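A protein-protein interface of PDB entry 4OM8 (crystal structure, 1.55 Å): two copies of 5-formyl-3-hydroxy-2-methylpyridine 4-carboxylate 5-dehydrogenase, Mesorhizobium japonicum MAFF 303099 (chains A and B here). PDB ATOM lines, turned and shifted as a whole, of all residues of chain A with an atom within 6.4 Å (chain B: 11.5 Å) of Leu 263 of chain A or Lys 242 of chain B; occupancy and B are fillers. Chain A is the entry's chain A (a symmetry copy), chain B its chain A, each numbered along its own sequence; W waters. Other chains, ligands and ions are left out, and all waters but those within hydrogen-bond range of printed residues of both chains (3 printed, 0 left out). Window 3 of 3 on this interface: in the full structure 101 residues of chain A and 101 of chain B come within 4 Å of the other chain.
The backbone carbonyl oxygen of Asp 239 of chain B sits at hydrogen-bond distance from the side-chain hydroxyl of Ser 243 of chain B (3.1 Å).
The side-chain hydroxyl (OG) of Ser 245 of chain B sits at hydrogen-bond distance from the backbone carbonyl oxygen (O) of Tyr 241 of chain B (2.8 Å).
The backbone carbonyl oxygen (O) of Val 262 of chain A sits at hydrogen-bond distance from the side-chain hydroxyl (OG1) of Thr 266 of chain A (2.9 Å).
The backbone carbonyl oxygen (O) of Lys 242 of chain B is in hydrogen-bond range of the side-chain hydroxyl (OG) of Ser 245 of chain B (3.5 Å).
O of Ser 243 of chain B lies within hydrogen-bond range of OG of Ser 246 of chain B, at 2.5 Å.
The side-chain hydroxyl of Thr 266 of chain A sits at hydrogen-bond distance from the backbone carbonyl oxygen of Leu 263 of chain A (3.2 Å).
OH of Tyr 192 of chain A touches CB of Val 244 of chain B, 3.3 Å away.
Tyr 192 of chain A touches Ser 245 of chain B (CE2 to N, 3.8 Å).
Val 258 of chain A touches Lys 242 of chain B (CG2 to O, 3.6 Å).
CG2 of Val 258 of chain A touches OG of Ser 245 of chain B, at 3.99 Å.
CG2 of Val 258 of chain A touches CB of Ser 246 of chain B, at 3.6 Å.
Tyr 241 of chain B touches Val 262 of chain A (CE2 to CG2, 3.8 Å).
Leu 263 of chain A touches Lys 242 of chain B.
Thr 266 of chain A touches Leu 238 of chain B.
Thr 266 of chain A touches Asp 239 of chain B.
Lys 242 of chain B touches Thr 266 of chain A (CD to OG1, 3.4 Å).
Of chain B, only Lys 242 comes within 4 Å of Leu 263 of chain A.
Of chain A, only Val 258 (3.6 Å), Val 262 (3.9 Å), Leu 263 (3.8 Å) and Thr 266 (3.4 Å) come within 4 Å of Lys 242 of chain B.
No residue of chain B comes within 4 Å of Ala 259 of chain A.
No residue of chain B comes within 4 Å of Pro 260 of chain A.
Val 262 of chain A touches just these residues of chain B: Tyr 241 and Lys 242.
Printed residues of chain B within 4 Å of Thr 266 of chain A: Leu 238, Asp 239 and Lys 242.
Of the printed residues of chain A, Leu 248 of chain B touches Tyr 192 (3.6 Å).
Printed residues of chain A within 4 Å of Leu 238 of chain B: Lys 265 (3.7 Å) and Thr 266 (3.4 Å).
Asp 234 of chain B touches none of the printed residues of chain A.
Met 230 of chain B touches none of the printed residues of chain A.
The nearest printed residue of chain B that does not touch Val 258 of chain A is Asn 249 of chain B (4.9 Å).
Hydrophobic or aromatic side chains of chain B within 4 Å of the printed part of chain A: Leu 238, Tyr 241, Val 244 and Leu 248.
Along chain B the printed residues that touch a printed residue of chain A span positions 238 to 248.
Of the 12 printed residues of chain A, 6 touch a printed residue of chain B.
Printed residues of chain A that touch a printed residue of chain B: Tyr 192, Val 258, Val 262, Leu 263, Lys 265 and Thr 266.
Hydrophobic or aromatic side chains of chain A that line the printed part of chain B: Tyr 192, Val 258, Val 262 and Leu 263.
Among the printed residues, 14 pairs touch across the chains.
Among the printed residues, no Asp or Glu carboxylate lies within 4 Å of a Lys or Arg side-chain nitrogen of the other chain.
No position is printed for both chains.
Water W2 lies within hydrogen-bond range of the side-chain amino group of Lys 242 of chain B (2.6 Å), the side-chain hydroxyl of Thr 266 of chain A (3.0 Å) and the backbone carbonyl oxygen of Leu 263 of chain A (3.0 Å).
Water W3 lies within hydrogen-bond range of OH of Tyr 241 of chain B (2.6 Å), OD1 of Asn 249 of chain B (2.8 Å) and O of Tyr 192 of chain A (2.8 Å).
Water W1 bridges N of Ala 259 of chain A (2.9 Å) and OG of Ser 245 of chain B (2.9 Å).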
ATOM      1  N   TYR A 192     -29.684   5.026  16.003  1.00  0.00           N
ATOM      2  CA  TYR A 192     -28.941   4.123  16.869  1.00  0.00           C
ATOM      3  C   TYR A 192     -27.512   3.925  16.361  1.00  0.00           C
ATOM      4  O   TYR A 192     -26.621   3.651  17.150  1.00  0.00           O
ATOM      5  CB  TYR A 192     -29.687   2.781  17.039  1.00  0.00           C
ATOM      6  CG  TYR A 192     -30.651   2.844  18.213  1.00  0.00           C
ATOM      7  CD1 TYR A 192     -31.736   3.709  18.210  1.00  0.00           C
ATOM      8  CD2 TYR A 192     -30.447   2.067  19.344  1.00  0.00           C
ATOM      9  CE1 TYR A 192     -32.600   3.785  19.306  1.00  0.00           C
ATOM     10  CE2 TYR A 192     -31.290   2.134  20.430  1.00  0.00           C
ATOM     11  CZ  TYR A 192     -32.361   2.985  20.412  1.00  0.00           C
ATOM     12  OH  TYR A 192     -33.183   3.016  21.520  1.00  0.00           O
ATOM     13  N   VAL A 258     -25.315  -4.275  24.531  1.00  0.00           N
ATOM     14  CA  VAL A 258     -25.500  -3.061  25.323  1.00  0.00           C
ATOM     15  C   VAL A 258     -24.147  -2.573  25.833  1.00  0.00           C
ATOM     16  O   VAL A 258     -23.330  -3.362  26.304  1.00  0.00           O
ATOM     17  CB  VAL A 258     -26.463  -3.281  26.510  1.00  0.00           C
ATOM     18  CG1 VAL A 258     -26.726  -1.962  27.242  1.00  0.00           C
ATOM     19  CG2 VAL A 258     -27.759  -3.868  26.024  1.00  0.00           C
ATOM     20  N   ALA A 259     -23.902  -1.274  25.700  1.00  0.00           N
ATOM     21  CA  ALA A 259     -22.660  -0.671  26.171  1.00  0.00           C
ATOM     22  C   ALA A 259     -22.548  -0.774  27.683  1.00  0.00           C
ATOM     23  O   ALA A 259     -23.538  -0.574  28.394  1.00  0.00           O
ATOM     24  CB  ALA A 259     -22.587   0.786  25.741  1.00  0.00           C
ATOM     25  N   PRO A 260     -21.346  -1.091  28.187  1.00  0.00           N
ATOM     26  CA  PRO A 260     -21.136  -1.186  29.637  1.00  0.00           C
ATOM     27  C   PRO A 260     -21.628   0.024  30.438  1.00  0.00           C
ATOM     28  O   PRO A 260     -22.209  -0.164  31.512  1.00  0.00           O
ATOM     29  CB  PRO A 260     -19.619  -1.320  29.749  1.00  0.00           C
ATOM     30  CG  PRO A 260     -19.237  -2.063  28.504  1.00  0.00           C
ATOM     31  CD  PRO A 260     -20.182  -1.574  27.421  1.00  0.00           C
ATOM     32  N   MET A 261     -21.415   1.232  29.927  1.00  0.00           N
ATOM     33  CA  MET A 261     -21.835   2.436  30.632  1.00  0.00           C
ATOM     34  C   MET A 261     -23.358   2.491  30.751  1.00  0.00           C
ATOM     35  O   MET A 261     -23.901   2.948  31.756  1.00  0.00           O
ATOM     36  CB  MET A 261     -21.311   3.682  29.913  1.00  0.00           C
ATOM     37  CG  MET A 261     -21.809   4.997  30.486  1.00  0.00           C
ATOM     38  SD  MET A 261     -21.116   6.432  29.622  1.00  0.00           S
ATOM     39  CE  MET A 261     -21.663   6.189  27.946  1.00  0.00           C
ATOM     40  N   VAL A 262     -24.052   2.014  29.725  1.00  0.00           N
ATOM     41  CA  VAL A 262     -25.512   1.989  29.770  1.00  0.00           C
ATOM     42  C   VAL A 262     -25.998   0.935  30.777  1.00  0.00           C
ATOM     43  O   VAL A 262     -26.960   1.178  31.511  1.00  0.00           O
ATOM     44  CB  VAL A 262     -26.107   1.717  28.360  1.00  0.00           C
ATOM     45  CG1 VAL A 262     -27.616   1.458  28.406  1.00  0.00           C
ATOM     46  CG2 VAL A 262     -25.815   2.892  27.443  1.00  0.00           C
ATOM     47  N   LEU A 263     -25.334  -0.225  30.816  1.00  0.00           N
ATOM     48  CA  LEU A 263     -25.656  -1.240  31.824  1.00  0.00           C
ATOM     49  C   LEU A 263     -25.413  -0.700  33.232  1.00  0.00           C
ATOM     50  O   LEU A 263     -26.194  -0.941  34.142  1.00  0.00           O
ATOM     51  CB  LEU A 263     -24.833  -2.518  31.592  1.00  0.00           C
ATOM     52  CG  LEU A 263     -25.215  -3.284  30.327  1.00  0.00           C
ATOM     53  CD1 LEU A 263     -24.254  -4.447  30.083  1.00  0.00           C
ATOM     54  CD2 LEU A 263     -26.661  -3.777  30.402  1.00  0.00           C
ATOM     55  N   GLU A 264     -24.327   0.047  33.406  1.00  0.00           N
ATOM     56  CA  GLU A 264     -23.990   0.614  34.708  1.00  0.00           C
ATOM     57  C   GLU A 264     -25.040   1.622  35.177  1.00  0.00           C
ATOM     58  O   GLU A 264     -25.488   1.577  36.325  1.00  0.00           O
ATOM     59  CB  GLU A 264     -22.605   1.272  34.656  1.00  0.00           C
ATOM     60  CG  GLU A 264     -22.142   1.843  35.986  1.00  0.00           C
ATOM     61  CD  GLU A 264     -20.709   2.335  35.947  1.00  0.00           C
ATOM     62  OE1 GLU A 264     -20.060   2.345  37.014  1.00  0.00           O
ATOM     63  OE2 GLU A 264     -20.236   2.718  34.857  1.00  0.00           O
ATOM     64  N   LYS A 265     -25.438   2.528  34.284  1.00  0.00           N
ATOM     65  CA  LYS A 265     -26.432   3.540  34.627  1.00  0.00           C
ATOM     66  C   LYS A 265     -27.758   2.896  34.988  1.00  0.00           C
ATOM     67  O   LYS A 265     -28.365   3.219  36.013  1.00  0.00           O
ATOM     68  CB  LYS A 265     -26.634   4.529  33.466  1.00  0.00           C
ATOM     69  CG  LYS A 265     -25.435   5.405  33.158  1.00  0.00           C
ATOM     70  CD  LYS A 265     -25.316   6.573  34.107  1.00  0.00           C
ATOM     71  CE  LYS A 265     -24.210   7.528  33.647  1.00  0.00           C
ATOM     72  NZ  LYS A 265     -24.114   8.705  34.547  1.00  0.00           N
ATOM     73  N   THR A 266     -28.212   1.969  34.152  1.00  0.00           N
ATOM     74  CA  THR A 266     -29.531   1.365  34.373  1.00  0.00           C
ATOM     75  C   THR A 266     -29.524   0.480  35.620  1.00  0.00           C
ATOM     76  O   THR A 266     -30.518   0.419  36.347  1.00  0.00           O
ATOM     77  CB  THR A 266     -30.005   0.546  33.161  1.00  0.00           C
ATOM     78  OG1 THR A 266     -28.992  -0.390  32.778  1.00  0.00           O
ATOM     79  CG2 THR A 266     -30.336   1.480  31.976  1.00  0.00           C
ATOM     80  N   SER A 267     -28.397  -0.178  35.881  1.00  0.00           N
ATOM     81  CA  SER A 267     -28.278  -1.017  37.072  1.00  0.00           C
ATOM     82  C   SER A 267     -28.411  -0.156  38.322  1.00  0.00           C
ATOM     83  O   SER A 267     -28.976  -0.588  39.331  1.00  0.00           O
ATOM     84  CB  SER A 267     -26.946  -1.765  37.076  1.00  0.00           C
ATOM     85  OG  SER A 267     -26.789  -2.543  38.258  1.00  0.00           O
ATOM     86  N   ALA A 268     -27.910   1.074  38.240  1.00  0.00           N
ATOM     87  CA  ALA A 268     -27.975   2.008  39.363  1.00  0.00           C
ATOM     88  C   ALA A 268     -29.277   2.812  39.372  1.00  0.00           C
ATOM     89  O   ALA A 268     -29.408   3.768  40.141  1.00  0.00           O
ATOM     90  CB  ALA A 268     -26.765   2.949  39.337  1.00  0.00           C
ATOM     91  N   PRO B 229     -27.177  14.054  21.745  1.00  0.00           N
ATOM     92  CA  PRO B 229     -27.409  12.613  21.945  1.00  0.00           C
ATOM     93  C   PRO B 229     -27.460  12.139  23.409  1.00  0.00           C
ATOM     94  O   PRO B 229     -28.298  11.291  23.715  1.00  0.00           O
ATOM     95  CB  PRO B 229     -26.213  11.960  21.234  1.00  0.00           C
ATOM     96  CG  PRO B 229     -25.716  12.976  20.262  1.00  0.00           C
ATOM     97  CD  PRO B 229     -26.042  14.330  20.840  1.00  0.00           C
ATOM     98  N   MET B 230     -26.588  12.632  24.282  1.00  0.00           N
ATOM     99  CA  MET B 230     -26.609  12.161  25.666  1.00  0.00           C
ATOM    100  C   MET B 230     -27.886  12.661  26.346  1.00  0.00           C
ATOM    101  O   MET B 230     -28.574  11.911  27.044  1.00  0.00           O
ATOM    102  CB  MET B 230     -25.351  12.616  26.413  1.00  0.00           C
ATOM    103  CG  MET B 230     -24.041  12.059  25.831  1.00  0.00           C
ATOM    104  SD  MET B 230     -23.961  10.238  25.826  1.00  0.00           S
ATOM    105  CE  MET B 230     -24.267   9.907  24.109  1.00  0.00           C
ATOM    106  N   LEU B 232     -30.590  13.323  24.777  1.00  0.00           N
ATOM    107  CA  LEU B 232     -31.692  12.624  24.137  1.00  0.00           C
ATOM    108  C   LEU B 232     -31.891  11.241  24.766  1.00  0.00           C
ATOM    109  O   LEU B 232     -33.028  10.805  24.966  1.00  0.00           O
ATOM    110  CB  LEU B 232     -31.446  12.494  22.626  1.00  0.00           C
ATOM    111  CG  LEU B 232     -32.622  11.929  21.826  1.00  0.00           C
ATOM    112  CD1 LEU B 232     -33.785  12.909  21.846  1.00  0.00           C
ATOM    113  CD2 LEU B 232     -32.235  11.587  20.390  1.00  0.00           C
ATOM    114  N   LEU B 233     -30.793  10.543  25.054  1.00  0.00           N
ATOM    115  CA  LEU B 233     -30.869   9.292  25.804  1.00  0.00           C
ATOM    116  C   LEU B 233     -31.604   9.503  27.128  1.00  0.00           C
ATOM    117  O   LEU B 233     -32.453   8.690  27.504  1.00  0.00           O
ATOM    118  CB  LEU B 233     -29.469   8.725  26.062  1.00  0.00           C
ATOM    119  CG  LEU B 233     -28.744   8.183  24.830  1.00  0.00           C
ATOM    120  CD1 LEU B 233     -27.345   7.706  25.201  1.00  0.00           C
ATOM    121  CD2 LEU B 233     -29.540   7.055  24.158  1.00  0.00           C
ATOM    122  N   ASP B 234     -31.300  10.601  27.821  1.00  0.00           N
ATOM    123  CA  ASP B 234     -31.979  10.895  29.083  1.00  0.00           C
ATOM    124  C   ASP B 234     -33.478  11.138  28.878  1.00  0.00           C
ATOM    125  O   ASP B 234     -34.280  10.777  29.730  1.00  0.00           O
ATOM    126  CB  ASP B 234     -31.342  12.098  29.779  1.00  0.00           C
ATOM    127  CG  ASP B 234     -30.057  11.745  30.485  1.00  0.00           C
ATOM    128  OD1 ASP B 234     -29.710  10.535  30.554  1.00  0.00           O
ATOM    129  OD2 ASP B 234     -29.406  12.691  30.966  1.00  0.00           O
ATOM    130  N   MET B 235     -33.859  11.739  27.750  1.00  0.00           N
ATOM    131  CA  MET B 235     -35.274  11.969  27.461  1.00  0.00           C
ATOM    132  C   MET B 235     -35.999  10.676  27.130  1.00  0.00           C
ATOM    133  O   MET B 235     -37.122  10.453  27.583  1.00  0.00           O
ATOM    134  CB  MET B 235     -35.442  12.936  26.291  1.00  0.00           C
ATOM    135  CG  MET B 235     -35.043  14.350  26.571  1.00  0.00           C
ATOM    136  SD  MET B 235     -35.220  15.293  25.054  1.00  0.00           S
ATOM    137  CE  MET B 235     -36.848  14.767  24.581  1.00  0.00           C
ATOM    138  N   ALA B 236     -35.369   9.841  26.310  1.00  0.00           N
ATOM    139  CA  ALA B 236     -35.971   8.589  25.874  1.00  0.00           C
ATOM    140  C   ALA B 236     -36.038   7.601  27.021  1.00  0.00           C
ATOM    141  O   ALA B 236     -36.939   6.766  27.087  1.00  0.00           O
ATOM    142  CB  ALA B 236     -35.182   7.990  24.709  1.00  0.00           C
ATOM    143  N   GLY B 237     -35.062   7.700  27.913  1.00  0.00           N
ATOM    144  CA  GLY B 237     -34.913   6.750  29.003  1.00  0.00           C
ATOM    145  C   GLY B 237     -33.784   5.782  28.708  1.00  0.00           C
ATOM    146  O   GLY B 237     -33.770   5.121  27.666  1.00  0.00           O
ATOM    147  N   LEU B 238     -32.815   5.690  29.618  1.00  0.00           N
ATOM    148  CA  LEU B 238     -31.704   4.775  29.377  1.00  0.00           C
ATOM    149  C   LEU B 238     -32.161   3.317  29.474  1.00  0.00           C
ATOM    150  O   LEU B 238     -31.516   2.423  28.902  1.00  0.00           O
ATOM    151  CB  LEU B 238     -30.553   5.056  30.349  1.00  0.00           C
ATOM    152  CG  LEU B 238     -29.817   6.389  30.152  1.00  0.00           C
ATOM    153  CD1 LEU B 238     -28.740   6.589  31.209  1.00  0.00           C
ATOM    154  CD2 LEU B 238     -29.197   6.429  28.781  1.00  0.00           C
ATOM    155  N   ASP B 239     -33.269   3.077  30.180  1.00  0.00           N
ATOM    156  CA  ASP B 239     -33.869   1.750  30.206  1.00  0.00           C
ATOM    157  C   ASP B 239     -34.348   1.363  28.809  1.00  0.00           C
ATOM    158  O   ASP B 239     -34.169   0.225  28.368  1.00  0.00           O
ATOM    159  CB  ASP B 239     -35.020   1.691  31.232  1.00  0.00           C
ATOM    160  CG  ASP B 239     -36.047   2.808  31.060  1.00  0.00           C
ATOM    161  OD1 ASP B 239     -35.708   3.907  30.575  1.00  0.00           O
ATOM    162  OD2 ASP B 239     -37.214   2.594  31.460  1.00  0.00           O
ATOM    163  N   ILE B 240     -34.933   2.325  28.103  1.00  0.00           N
ATOM    164  CA  ILE B 240     -35.395   2.083  26.743  1.00  0.00           C
ATOM    165  C   ILE B 240     -34.204   1.873  25.806  1.00  0.00           C
ATOM    166  O   ILE B 240     -34.175   0.930  25.003  1.00  0.00           O
ATOM    167  CB  ILE B 240     -36.261   3.247  26.247  1.00  0.00           C
ATOM    168  CG1 ILE B 240     -37.515   3.392  27.126  1.00  0.00           C
ATOM    169  CG2 ILE B 240     -36.606   3.059  24.770  1.00  0.00           C
ATOM    170  CD1 ILE B 240     -38.311   2.126  27.291  1.00  0.00           C
ATOM    171  N   TYR B 241     -33.205   2.736  25.929  1.00  0.00           N
ATOM    172  CA  TYR B 241     -32.009   2.592  25.104  1.00  0.00           C
ATOM    173  C   TYR B 241     -31.339   1.241  25.345  1.00  0.00           C
ATOM    174  O   TYR B 241     -30.894   0.605  24.403  1.00  0.00           O
ATOM    175  CB  TYR B 241     -31.019   3.726  25.359  1.00  0.00           C
ATOM    176  CG  TYR B 241     -29.824   3.657  24.433  1.00  0.00           C
ATOM    177  CD1 TYR B 241     -29.982   3.732  23.044  1.00  0.00           C
ATOM    178  CD2 TYR B 241     -28.543   3.493  24.938  1.00  0.00           C
ATOM    179  CE1 TYR B 241     -28.878   3.657  22.190  1.00  0.00           C
ATOM    180  CE2 TYR B 241     -27.439   3.405  24.100  1.00  0.00           C
ATOM    181  CZ  TYR B 241     -27.611   3.496  22.735  1.00  0.00           C
ATOM    182  OH  TYR B 241     -26.499   3.399  21.925  1.00  0.00           O
ATOM    183  N   LYS B 242     -31.266   0.803  26.601  1.00  0.00           N
ATOM    184  CA  LYS B 242     -30.756  -0.538  26.897  1.00  0.00           C
ATOM    185  C   LYS B 242     -31.567  -1.628  26.171  1.00  0.00           C
ATOM    186  O   LYS B 242     -31.001  -2.459  25.459  1.00  0.00           O
ATOM    187  CB  LYS B 242     -30.762  -0.785  28.410  1.00  0.00           C
ATOM    188  CG  LYS B 242     -30.473  -2.224  28.844  1.00  0.00           C
ATOM    189  CD  LYS B 242     -30.485  -2.319  30.368  1.00  0.00           C
ATOM    190  CE  LYS B 242     -30.387  -3.767  30.840  1.00  0.00           C
ATOM    191  NZ  LYS B 242     -30.333  -3.829  32.344  1.00  0.00           N
ATOM    192  N   SER B 243     -32.882  -1.612  26.347  1.00  0.00           N
ATOM    193  CA  SER B 243     -33.740  -2.635  25.755  1.00  0.00           C
ATOM    194  C   SER B 243     -33.602  -2.691  24.247  1.00  0.00           C
ATOM    195  O   SER B 243     -33.466  -3.769  23.668  1.00  0.00           O
ATOM    196  CB  SER B 243     -35.202  -2.375  26.116  1.00  0.00           C
ATOM    197  OG  SER B 243     -35.396  -2.440  27.514  1.00  0.00           O
ATOM    198  N   VAL B 244     -33.639  -1.529  23.607  1.00  0.00           N
ATOM    199  CA  VAL B 244     -33.594  -1.499  22.150  1.00  0.00           C
ATOM    200  C   VAL B 244     -32.200  -1.801  21.617  1.00  0.00           C
ATOM    201  O   VAL B 244     -32.044  -2.607  20.695  1.00  0.00           O
ATOM    202  CB  VAL B 244     -34.067  -0.150  21.609  1.00  0.00           C
ATOM    203  CG1 VAL B 244     -33.946  -0.109  20.094  1.00  0.00           C
ATOM    204  CG2 VAL B 244     -35.514   0.077  22.026  1.00  0.00           C
ATOM    205  N   SER B 245     -31.180  -1.175  22.198  1.00  0.00           N
ATOM    206  CA  SER B 245     -29.826  -1.363  21.686  1.00  0.00           C
ATOM    207  C   SER B 245     -29.375  -2.808  21.870  1.00  0.00           C
ATOM    208  O   SER B 245     -28.521  -3.282  21.119  1.00  0.00           O
ATOM    209  CB  SER B 245     -28.836  -0.395  22.345  1.00  0.00           C
ATOM    210  OG  SER B 245     -28.585  -0.726  23.700  1.00  0.00           O
ATOM    211  N   SER B 246     -29.965  -3.514  22.834  1.00  0.00           N
ATOM    212  CA  SER B 246     -29.614  -4.910  23.091  1.00  0.00           C
ATOM    213  C   SER B 246     -29.813  -5.805  21.866  1.00  0.00           C
ATOM    214  O   SER B 246     -29.113  -6.806  21.703  1.00  0.00           O
ATOM    215  CB  SER B 246     -30.417  -5.461  24.281  1.00  0.00           C
ATOM    216  OG  SER B 246     -31.797  -5.642  23.990  1.00  0.00           O
ATOM    217  N   PHE B 247     -30.774  -5.464  21.011  1.00  0.00           N
ATOM    218  CA  PHE B 247     -30.943  -6.235  19.780  1.00  0.00           C
ATOM    219  C   PHE B 247     -30.628  -5.405  18.544  1.00  0.00           C
ATOM    220  O   PHE B 247     -30.193  -5.956  17.533  1.00  0.00           O
ATOM    221  CB  PHE B 247     -32.359  -6.829  19.672  1.00  0.00           C
ATOM    222  CG  PHE B 247     -33.448  -5.811  19.493  1.00  0.00           C
ATOM    223  CD1 PHE B 247     -33.800  -5.354  18.228  1.00  0.00           C
ATOM    224  CD2 PHE B 247     -34.146  -5.340  20.589  1.00  0.00           C
ATOM    225  CE1 PHE B 247     -34.806  -4.427  18.067  1.00  0.00           C
ATOM    226  CE2 PHE B 247     -35.164  -4.416  20.439  1.00  0.00           C
ATOM    227  CZ  PHE B 247     -35.493  -3.956  19.178  1.00  0.00           C
ATOM    228  N   LEU B 248     -30.813  -4.087  18.604  1.00  0.00           N
ATOM    229  CA  LEU B 248     -30.628  -3.296  17.389  1.00  0.00           C
ATOM    230  C   LEU B 248     -29.146  -3.082  17.062  1.00  0.00           C
ATOM    231  O   LEU B 248     -28.780  -3.075  15.890  1.00  0.00           O
ATOM    232  CB  LEU B 248     -31.362  -1.953  17.489  1.00  0.00           C
ATOM    233  CG  LEU B 248     -31.403  -1.100  16.213  1.00  0.00           C
ATOM    234  CD1 LEU B 248     -31.937  -1.929  15.043  1.00  0.00           C
ATOM    235  CD2 LEU B 248     -32.255   0.142  16.402  1.00  0.00           C
ATOM    236  N   ASN B 249     -28.287  -2.906  18.069  1.00  0.00           N
ATOM    237  CA  ASN B 249     -26.851  -2.774  17.787  1.00  0.00           C
ATOM    238  C   ASN B 249     -26.322  -3.964  17.001  1.00  0.00           C
ATOM    239  O   ASN B 249     -25.477  -3.814  16.119  1.00  0.00           O
ATOM    240  CB  ASN B 249     -26.018  -2.627  19.070  1.00  0.00           C
ATOM    241  CG  ASN B 249     -26.037  -1.214  19.633  1.00  0.00           C
ATOM    242  OD1 ASN B 249     -26.525  -0.276  19.002  1.00  0.00           O
ATOM    243  ND2 ASN B 249     -25.496  -1.061  20.837  1.00  0.00           N
ATOM    244  N   ALA B 250     -26.842  -5.145  17.321  1.00  0.00           N
ATOM    245  CA  ALA B 250     -26.433  -6.359  16.636  1.00  0.00           C
ATOM    246  C   ALA B 250     -26.804  -6.351  15.157  1.00  0.00           C
ATOM    247  O   ALA B 250     -26.150  -7.020  14.357  1.00  0.00           O
ATOM    248  CB  ALA B 250     -27.047  -7.572  17.328  1.00  0.00           C
HETATM  249  O   HOH W   1     -26.000   0.337  24.533  1.00  0.00           O
HETATM  250  O   HOH W   2     -28.246  -3.094  33.722  1.00  0.00           O
HETATM  251  O   HOH W   3     -27.070   2.368  19.563  1.00  0.00           O
